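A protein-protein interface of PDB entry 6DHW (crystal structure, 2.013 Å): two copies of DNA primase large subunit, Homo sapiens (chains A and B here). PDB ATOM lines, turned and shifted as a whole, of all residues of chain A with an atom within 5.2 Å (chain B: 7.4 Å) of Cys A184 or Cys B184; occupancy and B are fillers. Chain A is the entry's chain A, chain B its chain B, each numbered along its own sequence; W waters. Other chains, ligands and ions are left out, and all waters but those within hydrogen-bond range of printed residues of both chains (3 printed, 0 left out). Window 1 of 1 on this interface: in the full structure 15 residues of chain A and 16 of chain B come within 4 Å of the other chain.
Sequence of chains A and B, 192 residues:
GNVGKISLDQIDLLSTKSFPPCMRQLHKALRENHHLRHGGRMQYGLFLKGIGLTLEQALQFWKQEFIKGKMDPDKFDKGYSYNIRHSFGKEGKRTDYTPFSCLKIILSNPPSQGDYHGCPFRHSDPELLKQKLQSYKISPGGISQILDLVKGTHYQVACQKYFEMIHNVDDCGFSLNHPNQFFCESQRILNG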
ATOM      1  N   GLY A  50      39.086   7.145 -20.356  1.00  0.00           N
ATOM      2  CA  GLY A  50      37.819   6.674 -19.825  1.00  0.00           C
ATOM      3  C   GLY A  50      37.115   5.672 -20.715  1.00  0.00           C
ATOM      4  O   GLY A  50      36.313   4.872 -20.221  1.00  0.00           O
ATOM      5  N   ASN A 180      32.224  11.255 -20.995  1.00  0.00           N
ATOM      6  CA  ASN A 180      32.253   9.812 -21.211  1.00  0.00           C
ATOM      7  C   ASN A 180      30.861   9.203 -21.086  1.00  0.00           C
ATOM      8  O   ASN A 180      30.562   8.187 -21.732  1.00  0.00           O
ATOM      9  CB  ASN A 180      33.225   9.158 -20.232  1.00  0.00           C
ATOM     10  CG  ASN A 180      34.676   9.448 -20.574  1.00  0.00           C
ATOM     11  OD1 ASN A 180      35.267  10.394 -20.057  1.00  0.00           O
ATOM     12  ND2 ASN A 180      35.249   8.644 -21.464  1.00  0.00           N
ATOM     13  N   GLN A 181      29.990   9.823 -20.287  1.00  0.00           N
ATOM     14  CA  GLN A 181      28.595   9.402 -20.257  1.00  0.00           C
ATOM     15  C   GLN A 181      27.923   9.679 -21.594  1.00  0.00           C
ATOM     16  O   GLN A 181      27.174   8.838 -22.108  1.00  0.00           O
ATOM     17  CB  GLN A 181      27.865  10.124 -19.125  1.00  0.00           C
ATOM     18  CG  GLN A 181      26.365   9.896 -19.086  1.00  0.00           C
ATOM     19  CD  GLN A 181      25.651  10.934 -18.237  1.00  0.00           C
ATOM     20  OE1 GLN A 181      26.169  12.028 -18.010  1.00  0.00           O
ATOM     21  NE2 GLN A 181      24.461  10.593 -17.757  1.00  0.00           N
ATOM     22  N   PHE A 182      28.180  10.859 -22.163  1.00  0.00           N
ATOM     23  CA  PHE A 182      27.749  11.166 -23.522  1.00  0.00           C
ATOM     24  C   PHE A 182      28.183  10.067 -24.484  1.00  0.00           C
ATOM     25  O   PHE A 182      27.377   9.567 -25.278  1.00  0.00           O
ATOM     26  CB  PHE A 182      28.327  12.525 -23.935  1.00  0.00           C
ATOM     27  CG  PHE A 182      27.814  13.058 -25.250  1.00  0.00           C
ATOM     28  CD1 PHE A 182      28.187  12.476 -26.455  1.00  0.00           C
ATOM     29  CD2 PHE A 182      27.000  14.179 -25.280  1.00  0.00           C
ATOM     30  CE1 PHE A 182      27.726  12.979 -27.658  1.00  0.00           C
ATOM     31  CE2 PHE A 182      26.540  14.690 -26.479  1.00  0.00           C
ATOM     32  CZ  PHE A 182      26.901  14.091 -27.668  1.00  0.00           C
ATOM     33  N   PHE A 183      29.461   9.681 -24.424  1.00  0.00           N
ATOM     34  CA  PHE A 183      29.963   8.643 -25.322  1.00  0.00           C
ATOM     35  C   PHE A 183      29.218   7.320 -25.143  1.00  0.00           C
ATOM     36  O   PHE A 183      28.800   6.697 -26.126  1.00  0.00           O
ATOM     37  CB  PHE A 183      31.462   8.433 -25.112  1.00  0.00           C
ATOM     38  CG  PHE A 183      32.038   7.351 -25.979  1.00  0.00           C
ATOM     39  CD1 PHE A 183      32.371   7.606 -27.301  1.00  0.00           C
ATOM     40  CD2 PHE A 183      32.234   6.072 -25.474  1.00  0.00           C
ATOM     41  CE1 PHE A 183      32.892   6.607 -28.103  1.00  0.00           C
ATOM     42  CE2 PHE A 183      32.758   5.068 -26.268  1.00  0.00           C
ATOM     43  CZ  PHE A 183      33.087   5.335 -27.584  1.00  0.00           C
ATOM     44  N   CYS A 184      29.082   6.853 -23.895  1.00  0.00           N
ATOM     45  CA  CYS A 184      28.425   5.566 -23.661  1.00  0.00           C
ATOM     46  C   CYS A 184      26.971   5.586 -24.131  1.00  0.00           C
ATOM     47  O   CYS A 184      26.485   4.608 -24.713  1.00  0.00           O
ATOM     48  CB  CYS A 184      28.512   5.165 -22.185  1.00  0.00           C
ATOM     49  SG  CYS A 184      30.176   4.686 -21.580  1.00  0.00           S
ATOM     50  N   GLU A 185      26.252   6.683 -23.879  1.00  0.00           N
ATOM     51  CA  GLU A 185      24.853   6.742 -24.297  1.00  0.00           C
ATOM     52  C   GLU A 185      24.730   6.820 -25.816  1.00  0.00           C
ATOM     53  O   GLU A 185      23.826   6.211 -26.410  1.00  0.00           O
ATOM     54  CB  GLU A 185      24.147   7.917 -23.623  1.00  0.00           C
ATOM     55  CG  GLU A 185      24.059   7.778 -22.105  1.00  0.00           C
ATOM     56  CD  GLU A 185      22.925   6.861 -21.659  1.00  0.00           C
ATOM     57  OE1 GLU A 185      22.179   6.363 -22.530  1.00  0.00           O
ATOM     58  OE2 GLU A 185      22.789   6.629 -20.435  1.00  0.00           O
ATOM     59  N   SER A 186      25.644   7.546 -26.468  1.00  0.00           N
ATOM     60  CA  SER A 186      25.653   7.576 -27.926  1.00  0.00           C
ATOM     61  C   SER A 186      25.890   6.185 -28.499  1.00  0.00           C
ATOM     62  O   SER A 186      25.185   5.749 -29.417  1.00  0.00           O
ATOM     63  CB  SER A 186      26.723   8.543 -28.432  1.00  0.00           C
ATOM     64  OG  SER A 186      26.967   8.333 -29.815  1.00  0.00           O
ATOM     65  N   GLN A 187      26.888   5.473 -27.967  1.00  0.00           N
ATOM     66  CA  GLN A 187      27.169   4.119 -28.437  1.00  0.00           C
ATOM     67  C   GLN A 187      25.994   3.187 -28.174  1.00  0.00           C
ATOM     68  O   GLN A 187      25.701   2.304 -28.989  1.00  0.00           O
ATOM     69  CB  GLN A 187      28.439   3.589 -27.772  1.00  0.00           C
ATOM     70  CG  GLN A 187      29.729   4.202 -28.310  1.00  0.00           C
ATOM     71  CD  GLN A 187      30.052   3.742 -29.722  1.00  0.00           C
ATOM     72  OE1 GLN A 187      30.461   2.601 -29.929  1.00  0.00           O
ATOM     73  NE2 GLN A 187      29.872   4.627 -30.697  1.00  0.00           N
ATOM     74  N   ARG A 188      25.304   3.364 -27.044  1.00  0.00           N
ATOM     75  CA  ARG A 188      24.113   2.563 -26.783  1.00  0.00           C
ATOM     76  C   ARG A 188      23.064   2.792 -27.861  1.00  0.00           C
ATOM     77  O   ARG A 188      22.463   1.840 -28.372  1.00  0.00           O
ATOM     78  CB  ARG A 188      23.546   2.876 -25.401  1.00  0.00           C
ATOM     79  CG  ARG A 188      22.428   1.947 -25.005  1.00  0.00           C
ATOM     80  CD  ARG A 188      21.091   2.683 -25.041  1.00  0.00           C
ATOM     81  NE  ARG A 188      20.969   3.704 -24.002  1.00  0.00           N
ATOM     82  CZ  ARG A 188      20.546   3.458 -22.767  1.00  0.00           C
ATOM     83  NH1 ARG A 188      20.457   4.445 -21.885  1.00  0.00           N
ATOM     84  NH2 ARG A 188      20.229   2.217 -22.412  1.00  0.00           N
ATOM     85  N   ILE A 189      22.838   4.056 -28.228  1.00  0.00           N
ATOM     86  CA  ILE A 189      21.851   4.344 -29.268  1.00  0.00           C
ATOM     87  C   ILE A 189      22.290   3.736 -30.595  1.00  0.00           C
ATOM     88  O   ILE A 189      21.493   3.109 -31.304  1.00  0.00           O
ATOM     89  CB  ILE A 189      21.620   5.861 -29.390  1.00  0.00           C
ATOM     90  CG1 ILE A 189      20.896   6.397 -28.150  1.00  0.00           C
ATOM     91  CG2 ILE A 189      20.838   6.168 -30.654  1.00  0.00           C
ATOM     92  CD1 ILE A 189      19.563   5.728 -27.881  1.00  0.00           C
ATOM     93  N   SER B  18      35.169  -6.466 -16.792  1.00  0.00           N
ATOM     94  CA  SER B  18      34.291  -5.609 -17.577  1.00  0.00           C
ATOM     95  C   SER B  18      33.270  -6.354 -18.420  1.00  0.00           C
ATOM     96  O   SER B  18      32.390  -5.703 -18.993  1.00  0.00           O
ATOM     97  CB  SER B  18      35.112  -4.713 -18.519  1.00  0.00           C
ATOM     98  OG  SER B  18      35.794  -3.710 -17.799  1.00  0.00           O
ATOM     99  N   PHE B  47      29.765  -8.700 -29.889  1.00  0.00           N
ATOM    100  CA  PHE B  47      30.160  -7.930 -28.711  1.00  0.00           C
ATOM    101  C   PHE B  47      31.607  -7.447 -28.821  1.00  0.00           C
ATOM    102  O   PHE B  47      31.903  -6.270 -28.586  1.00  0.00           O
ATOM    103  CB  PHE B  47      29.967  -8.780 -27.459  1.00  0.00           C
ATOM    104  CG  PHE B  47      30.537  -8.168 -26.215  1.00  0.00           C
ATOM    105  CD1 PHE B  47      29.861  -7.155 -25.557  1.00  0.00           C
ATOM    106  CD2 PHE B  47      31.737  -8.621 -25.694  1.00  0.00           C
ATOM    107  CE1 PHE B  47      30.379  -6.593 -24.408  1.00  0.00           C
ATOM    108  CE2 PHE B  47      32.260  -8.065 -24.543  1.00  0.00           C
ATOM    109  CZ  PHE B  47      31.577  -7.048 -23.898  1.00  0.00           C
ATOM    110  N   ILE B  51      33.567  -3.524 -29.104  1.00  0.00           N
ATOM    111  CA  ILE B  51      34.634  -2.962 -28.284  1.00  0.00           C
ATOM    112  C   ILE B  51      35.898  -2.711 -29.093  1.00  0.00           C
ATOM    113  O   ILE B  51      36.885  -2.201 -28.546  1.00  0.00           O
ATOM    114  CB  ILE B  51      34.924  -3.832 -27.039  1.00  0.00           C
ATOM    115  CG1 ILE B  51      35.688  -5.105 -27.393  1.00  0.00           C
ATOM    116  CG2 ILE B  51      33.627  -4.185 -26.322  1.00  0.00           C
ATOM    117  CD1 ILE B  51      35.962  -5.987 -26.186  1.00  0.00           C
ATOM    118  N   PHE B 163      26.533  -5.491 -11.765  1.00  0.00           N
ATOM    119  CA  PHE B 163      27.485  -4.433 -12.100  1.00  0.00           C
ATOM    120  C   PHE B 163      27.871  -3.643 -10.857  1.00  0.00           C
ATOM    121  O   PHE B 163      29.061  -3.420 -10.583  1.00  0.00           O
ATOM    122  CB  PHE B 163      26.863  -3.518 -13.163  1.00  0.00           C
ATOM    123  CG  PHE B 163      27.727  -2.350 -13.565  1.00  0.00           C
ATOM    124  CD1 PHE B 163      27.778  -1.197 -12.793  1.00  0.00           C
ATOM    125  CD2 PHE B 163      28.460  -2.393 -14.737  1.00  0.00           C
ATOM    126  CE1 PHE B 163      28.561  -0.125 -13.169  1.00  0.00           C
ATOM    127  CE2 PHE B 163      29.245  -1.323 -15.119  1.00  0.00           C
ATOM    128  CZ  PHE B 163      29.294  -0.188 -14.335  1.00  0.00           C
ATOM    129  N   PHE B 174      22.767   4.277 -14.626  1.00  0.00           N
ATOM    130  CA  PHE B 174      22.303   4.194 -16.003  1.00  0.00           C
ATOM    131  C   PHE B 174      21.278   3.076 -16.113  1.00  0.00           C
ATOM    132  O   PHE B 174      21.171   2.216 -15.236  1.00  0.00           O
ATOM    133  CB  PHE B 174      23.465   3.959 -16.981  1.00  0.00           C
ATOM    134  CG  PHE B 174      24.166   2.642 -16.793  1.00  0.00           C
ATOM    135  CD1 PHE B 174      25.194   2.513 -15.874  1.00  0.00           C
ATOM    136  CD2 PHE B 174      23.801   1.534 -17.543  1.00  0.00           C
ATOM    137  CE1 PHE B 174      25.842   1.302 -15.703  1.00  0.00           C
ATOM    138  CE2 PHE B 174      24.444   0.322 -17.376  1.00  0.00           C
ATOM    139  CZ  PHE B 174      25.465   0.204 -16.456  1.00  0.00           C
ATOM    140  N   HIS B 178      22.003  -2.999 -23.076  1.00  0.00           N
ATOM    141  CA  HIS B 178      22.946  -3.490 -24.085  1.00  0.00           C
ATOM    142  C   HIS B 178      24.247  -3.947 -23.430  1.00  0.00           C
ATOM    143  O   HIS B 178      24.824  -3.192 -22.632  1.00  0.00           O
ATOM    144  CB  HIS B 178      23.247  -2.418 -25.134  1.00  0.00           C
ATOM    145  CG  HIS B 178      23.747  -2.974 -26.431  1.00  0.00           C
ATOM    146  ND1 HIS B 178      24.980  -3.576 -26.553  1.00  0.00           N
ATOM    147  CD2 HIS B 178      23.180  -3.023 -27.660  1.00  0.00           C
ATOM    148  CE1 HIS B 178      25.150  -3.976 -27.801  1.00  0.00           C
ATOM    149  NE2 HIS B 178      24.072  -3.651 -28.493  1.00  0.00           N
ATOM    150  N   PRO B 179      24.720  -5.162 -23.743  1.00  0.00           N
ATOM    151  CA  PRO B 179      25.992  -5.646 -23.167  1.00  0.00           C
ATOM    152  C   PRO B 179      27.178  -4.723 -23.401  1.00  0.00           C
ATOM    153  O   PRO B 179      28.043  -4.577 -22.523  1.00  0.00           O
ATOM    154  CB  PRO B 179      26.187  -7.000 -23.866  1.00  0.00           C
ATOM    155  CG  PRO B 179      24.801  -7.440 -24.221  1.00  0.00           C
ATOM    156  CD  PRO B 179      24.070  -6.177 -24.587  1.00  0.00           C
ATOM    157  N   ASN B 180      27.249  -4.105 -24.581  1.00  0.00           N
ATOM    158  CA  ASN B 180      28.351  -3.193 -24.855  1.00  0.00           C
ATOM    159  C   ASN B 180      28.242  -1.928 -24.013  1.00  0.00           C
ATOM    160  O   ASN B 180      29.264  -1.317 -23.677  1.00  0.00           O
ATOM    161  CB  ASN B 180      28.391  -2.864 -26.348  1.00  0.00           C
ATOM    162  CG  ASN B 180      28.917  -4.017 -27.182  1.00  0.00           C
ATOM    163  OD1 ASN B 180      28.153  -4.844 -27.677  1.00  0.00           O
ATOM    164  ND2 ASN B 180      30.233  -4.074 -27.344  1.00  0.00           N
ATOM    165  N   GLN B 181      27.022  -1.541 -23.633  1.00  0.00           N
ATOM    166  CA  GLN B 181      26.843  -0.449 -22.679  1.00  0.00           C
ATOM    167  C   GLN B 181      27.373  -0.828 -21.299  1.00  0.00           C
ATOM    168  O   GLN B 181      28.000  -0.005 -20.617  1.00  0.00           O
ATOM    169  CB  GLN B 181      25.365  -0.066 -22.613  1.00  0.00           C
ATOM    170  CG  GLN B 181      25.008   0.936 -21.535  1.00  0.00           C
ATOM    171  CD  GLN B 181      23.513   0.968 -21.267  1.00  0.00           C
ATOM    172  OE1 GLN B 181      22.799   0.012 -21.573  1.00  0.00           O
ATOM    173  NE2 GLN B 181      23.031   2.071 -20.698  1.00  0.00           N
ATOM    174  N   PHE B 182      27.098  -2.060 -20.862  1.00  0.00           N
ATOM    175  CA  PHE B 182      27.719  -2.592 -19.651  1.00  0.00           C
ATOM    176  C   PHE B 182      29.234  -2.433 -19.714  1.00  0.00           C
ATOM    177  O   PHE B 182      29.863  -1.923 -18.774  1.00  0.00           O
ATOM    178  CB  PHE B 182      27.320  -4.066 -19.491  1.00  0.00           C
ATOM    179  CG  PHE B 182      27.732  -4.697 -18.180  1.00  0.00           C
ATOM    180  CD1 PHE B 182      29.063  -4.976 -17.904  1.00  0.00           C
ATOM    181  CD2 PHE B 182      26.775  -5.060 -17.246  1.00  0.00           C
ATOM    182  CE1 PHE B 182      29.433  -5.570 -16.711  1.00  0.00           C
ATOM    183  CE2 PHE B 182      27.142  -5.657 -16.053  1.00  0.00           C
ATOM    184  CZ  PHE B 182      28.473  -5.911 -15.786  1.00  0.00           C
ATOM    185  N   PHE B 183      29.834  -2.862 -20.828  1.00  0.00           N
ATOM    186  CA  PHE B 183      31.284  -2.755 -20.984  1.00  0.00           C
ATOM    187  C   PHE B 183      31.749  -1.304 -20.898  1.00  0.00           C
ATOM    188  O   PHE B 183      32.750  -1.000 -20.239  1.00  0.00           O
ATOM    189  CB  PHE B 183      31.726  -3.377 -22.307  1.00  0.00           C
ATOM    190  CG  PHE B 183      33.209  -3.316 -22.531  1.00  0.00           C
ATOM    191  CD1 PHE B 183      34.045  -4.259 -21.957  1.00  0.00           C
ATOM    192  CD2 PHE B 183      33.772  -2.306 -23.296  1.00  0.00           C
ATOM    193  CE1 PHE B 183      35.414  -4.205 -22.155  1.00  0.00           C
ATOM    194  CE2 PHE B 183      35.140  -2.247 -23.498  1.00  0.00           C
ATOM    195  CZ  PHE B 183      35.961  -3.196 -22.926  1.00  0.00           C
ATOM    196  N   CYS B 184      31.057  -0.401 -21.601  1.00  0.00           N
ATOM    197  CA  CYS B 184      31.456   1.007 -21.627  1.00  0.00           C
ATOM    198  C   CYS B 184      31.427   1.620 -20.227  1.00  0.00           C
ATOM    199  O   CYS B 184      32.371   2.313 -19.819  1.00  0.00           O
ATOM    200  CB  CYS B 184      30.529   1.778 -22.574  1.00  0.00           C
ATOM    201  SG  CYS B 184      31.016   3.481 -23.003  1.00  0.00           S
ATOM    202  N   GLU B 185      30.368   1.345 -19.461  1.00  0.00           N
ATOM    203  CA  GLU B 185      30.265   1.934 -18.127  1.00  0.00           C
ATOM    204  C   GLU B 185      31.300   1.328 -17.185  1.00  0.00           C
ATOM    205  O   GLU B 185      31.867   2.028 -16.325  1.00  0.00           O
ATOM    206  CB  GLU B 185      28.852   1.759 -17.577  1.00  0.00           C
ATOM    207  CG  GLU B 185      27.772   2.449 -18.416  1.00  0.00           C
ATOM    208  CD  GLU B 185      27.687   3.953 -18.184  1.00  0.00           C
ATOM    209  OE1 GLU B 185      28.464   4.479 -17.359  1.00  0.00           O
ATOM    210  OE2 GLU B 185      26.835   4.606 -18.830  1.00  0.00           O
ATOM    211  N   SER B 186      31.571   0.027 -17.348  1.00  0.00           N
ATOM    212  CA  SER B 186      32.635  -0.602 -16.577  1.00  0.00           C
ATOM    213  C   SER B 186      33.976   0.060 -16.865  1.00  0.00           C
ATOM    214  O   SER B 186      34.737   0.361 -15.941  1.00  0.00           O
ATOM    215  CB  SER B 186      32.691  -2.101 -16.875  1.00  0.00           C
ATOM    216  OG  SER B 186      33.764  -2.704 -16.170  1.00  0.00           O
ATOM    217  N   GLN B 187      34.274   0.307 -18.145  1.00  0.00           N
ATOM    218  CA  GLN B 187      35.541   0.940 -18.500  1.00  0.00           C
ATOM    219  C   GLN B 187      35.632   2.336 -17.910  1.00  0.00           C
ATOM    220  O   GLN B 187      36.715   2.783 -17.515  1.00  0.00           O
ATOM    221  CB  GLN B 187      35.708   0.977 -20.018  1.00  0.00           C
ATOM    222  CG  GLN B 187      36.019  -0.388 -20.589  1.00  0.00           C
ATOM    223  CD  GLN B 187      37.387  -0.878 -20.174  1.00  0.00           C
ATOM    224  OE1 GLN B 187      38.406  -0.393 -20.660  1.00  0.00           O
ATOM    225  NE2 GLN B 187      37.417  -1.844 -19.267  1.00  0.00           N
ATOM    226  N   ARG B 188      34.501   3.042 -17.843  1.00  0.00           N
ATOM    227  CA  ARG B 188      34.501   4.337 -17.171  1.00  0.00           C
ATOM    228  C   ARG B 188      34.923   4.189 -15.715  1.00  0.00           C
ATOM    229  O   ARG B 188      35.763   4.949 -15.221  1.00  0.00           O
ATOM    230  CB  ARG B 188      33.120   4.988 -17.251  1.00  0.00           C
ATOM    231  CG  ARG B 188      32.778   5.611 -18.585  1.00  0.00           C
ATOM    232  CD  ARG B 188      31.443   6.328 -18.479  1.00  0.00           C
ATOM    233  NE  ARG B 188      31.467   7.357 -17.443  1.00  0.00           N
ATOM    234  CZ  ARG B 188      30.382   7.925 -16.927  1.00  0.00           C
ATOM    235  NH1 ARG B 188      29.173   7.560 -17.338  1.00  0.00           N
ATOM    236  NH2 ARG B 188      30.506   8.856 -15.992  1.00  0.00           N
ATOM    237  N   ILE B 189      34.352   3.208 -15.013  1.00  0.00           N
ATOM    238  CA  ILE B 189      34.685   3.049 -13.597  1.00  0.00           C
ATOM    239  C   ILE B 189      36.137   2.617 -13.406  1.00  0.00           C
ATOM    240  O   ILE B 189      36.850   3.160 -12.554  1.00  0.00           O
ATOM    241  CB  ILE B 189      33.709   2.073 -12.916  1.00  0.00           C
ATOM    242  CG1 ILE B 189      32.323   2.710 -12.820  1.00  0.00           C
ATOM    243  CG2 ILE B 189      34.215   1.689 -11.530  1.00  0.00           C
ATOM    244  CD1 ILE B 189      31.329   1.877 -12.071  1.00  0.00           C
ATOM    245  N   LEU B 190      36.601   1.637 -14.185  1.00  0.00           N
ATOM    246  CA  LEU B 190      37.932   1.081 -13.955  1.00  0.00           C
ATOM    247  C   LEU B 190      39.027   2.077 -14.301  1.00  0.00           C
ATOM    248  O   LEU B 190      40.117   2.023 -13.721  1.00  0.00           O
ATOM    249  CB  LEU B 190      38.116  -0.197 -14.770  1.00  0.00           C
ATOM    250  CG  LEU B 190      37.132  -1.332 -14.508  1.00  0.00           C
ATOM    251  CD1 LEU B 190      37.347  -2.422 -15.526  1.00  0.00           C
ATOM    252  CD2 LEU B 190      37.298  -1.871 -13.102  1.00  0.00           C
ATOM    253  N   ASN B 191      38.768   2.963 -15.255  1.00  0.00           N
ATOM    254  CA  ASN B 191      39.690   4.022 -15.633  1.00  0.00           C
ATOM    255  C   ASN B 191      39.331   5.354 -14.992  1.00  0.00           C
ATOM    256  O   ASN B 191      39.850   6.394 -15.407  1.00  0.00           O
ATOM    257  CB  ASN B 191      39.729   4.144 -17.155  1.00  0.00           C
ATOM    258  CG  ASN B 191      40.358   2.932 -17.811  1.00  0.00           C
ATOM    259  OD1 ASN B 191      41.429   2.482 -17.404  1.00  0.00           O
ATOM    260  ND2 ASN B 191      39.672   2.366 -18.801  1.00  0.00           N
HETATM  261  O   HOH W   1      24.863   4.372 -20.508  1.00  0.00           O
HETATM  262  O   HOH W   2      33.922   3.925 -21.562  1.00  0.00           O
HETATM  263  O   HOH W   3      26.112   0.030 -26.366  1.00  0.00           O
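The side-chain sulfur (SG) of Cys B184 is disulfide-bonded to the side-chain sulfur (SG) of Cys A184 (2.0 Å). The guanidinium group (NH2) of Arg A188 lies close to the side-chain amide nitrogen (NE2) of Gln B181, 3.3 Å away. The backbone carbonyl oxygen (O) of Gln B187 lies close to the backbone carbonyl oxygen (O) of Gly A50, at 3.4 Å.
The side-chain carboxylate (OE1) of Glu A185 lies within salt-bridge range of the guanidinium group (NH1) of Arg A188 (2.7 Å). The side-chain hydroxyl (OG) of Ser B18 lies within hydrogen-bond range of the side-chain amide nitrogen (NE2) of Gln B187, 2.9 Å away. The backbone NH (N) of His B178 sits at hydrogen-bond distance from the side-chain amide oxygen (OE1) of Gln B181, 3.5 Å away. NH1 of Arg B188 is in salt-bridge range of OE1 of Glu B185 (3.2 Å). The backbone carbonyl oxygen (O) of Gln B187 lies within hydrogen-bond range of the side-chain amide nitrogen (ND2) of Asn B191 (3.3 Å).
Among the printed residues, pairs that only touch across the chains: Gly A50 with Arg B188, Asn A180 with Arg B188, Gln A181 with Arg B188, Phe A183 with Cys B184, Cys A184 with Glu B185 and Cys A184 with Arg B188.
Cys A184 touches just these residues of chain B: Cys B184, Glu B185 and Arg B188. Of the printed residues of chain B, Arg A188 touches Gln B181. Of chain A, only Phe A183 and Cys A184 come within 4 Å of Cys B184. Printed residues of chain A within 4 Å of Gln B187: Gly A50 (3.4 Å). The nearest residue of chain B that does not touch Cys A184 is Gln B181 (5.1 Å).
Printed residues of chain A that touch a printed residue of chain B: Gly A50, Asn A180, Gln A181, Phe A183, Cys A184 and Arg A188. Hydrophobic or aromatic side chains of chain A that line the printed part of chain B: Phe A183. Among the printed residues, 9 pairs touch across the chains. Among the printed residues, no Asp or Glu carboxylate lies within 4 Å of a Lys or Arg side-chain nitrogen of the other chain.
Phe A183 touches Cys B184, but with the chains exchanged Cys A184 does not touch Phe B183 (6.2 Å). Cys A184 touches its own counterpart, Cys B184. Cys A184 touches Glu B185, but with the chains exchanged Glu A185 does not touch Cys B184 (5.8 Å). Cys A184 touches Arg B188, but with the chains exchanged Arg A188 does not touch Cys B184 (7.0 Å). 10 positions are printed for both chains.
Water W1 lies within hydrogen-bond range of the side-chain carboxylate (OE2) of Glu B185, the side-chain amide nitrogen (NE2) of Gln B181 and the side-chain carboxylate (OE2) of Glu A185. Water W2 lies within hydrogen-bond range of the backbone carbonyl oxygen of Cys B184 (2.8 Å) and the backbone carbonyl oxygen of Gly A50 (2.9 Å). Water W3 lies within hydrogen-bond range of the backbone NH of Gln B181 (3.3 Å), the backbone carbonyl oxygen of Gln A187 (3.5 Å) and the backbone NH of Arg A188 (3.5 Å).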
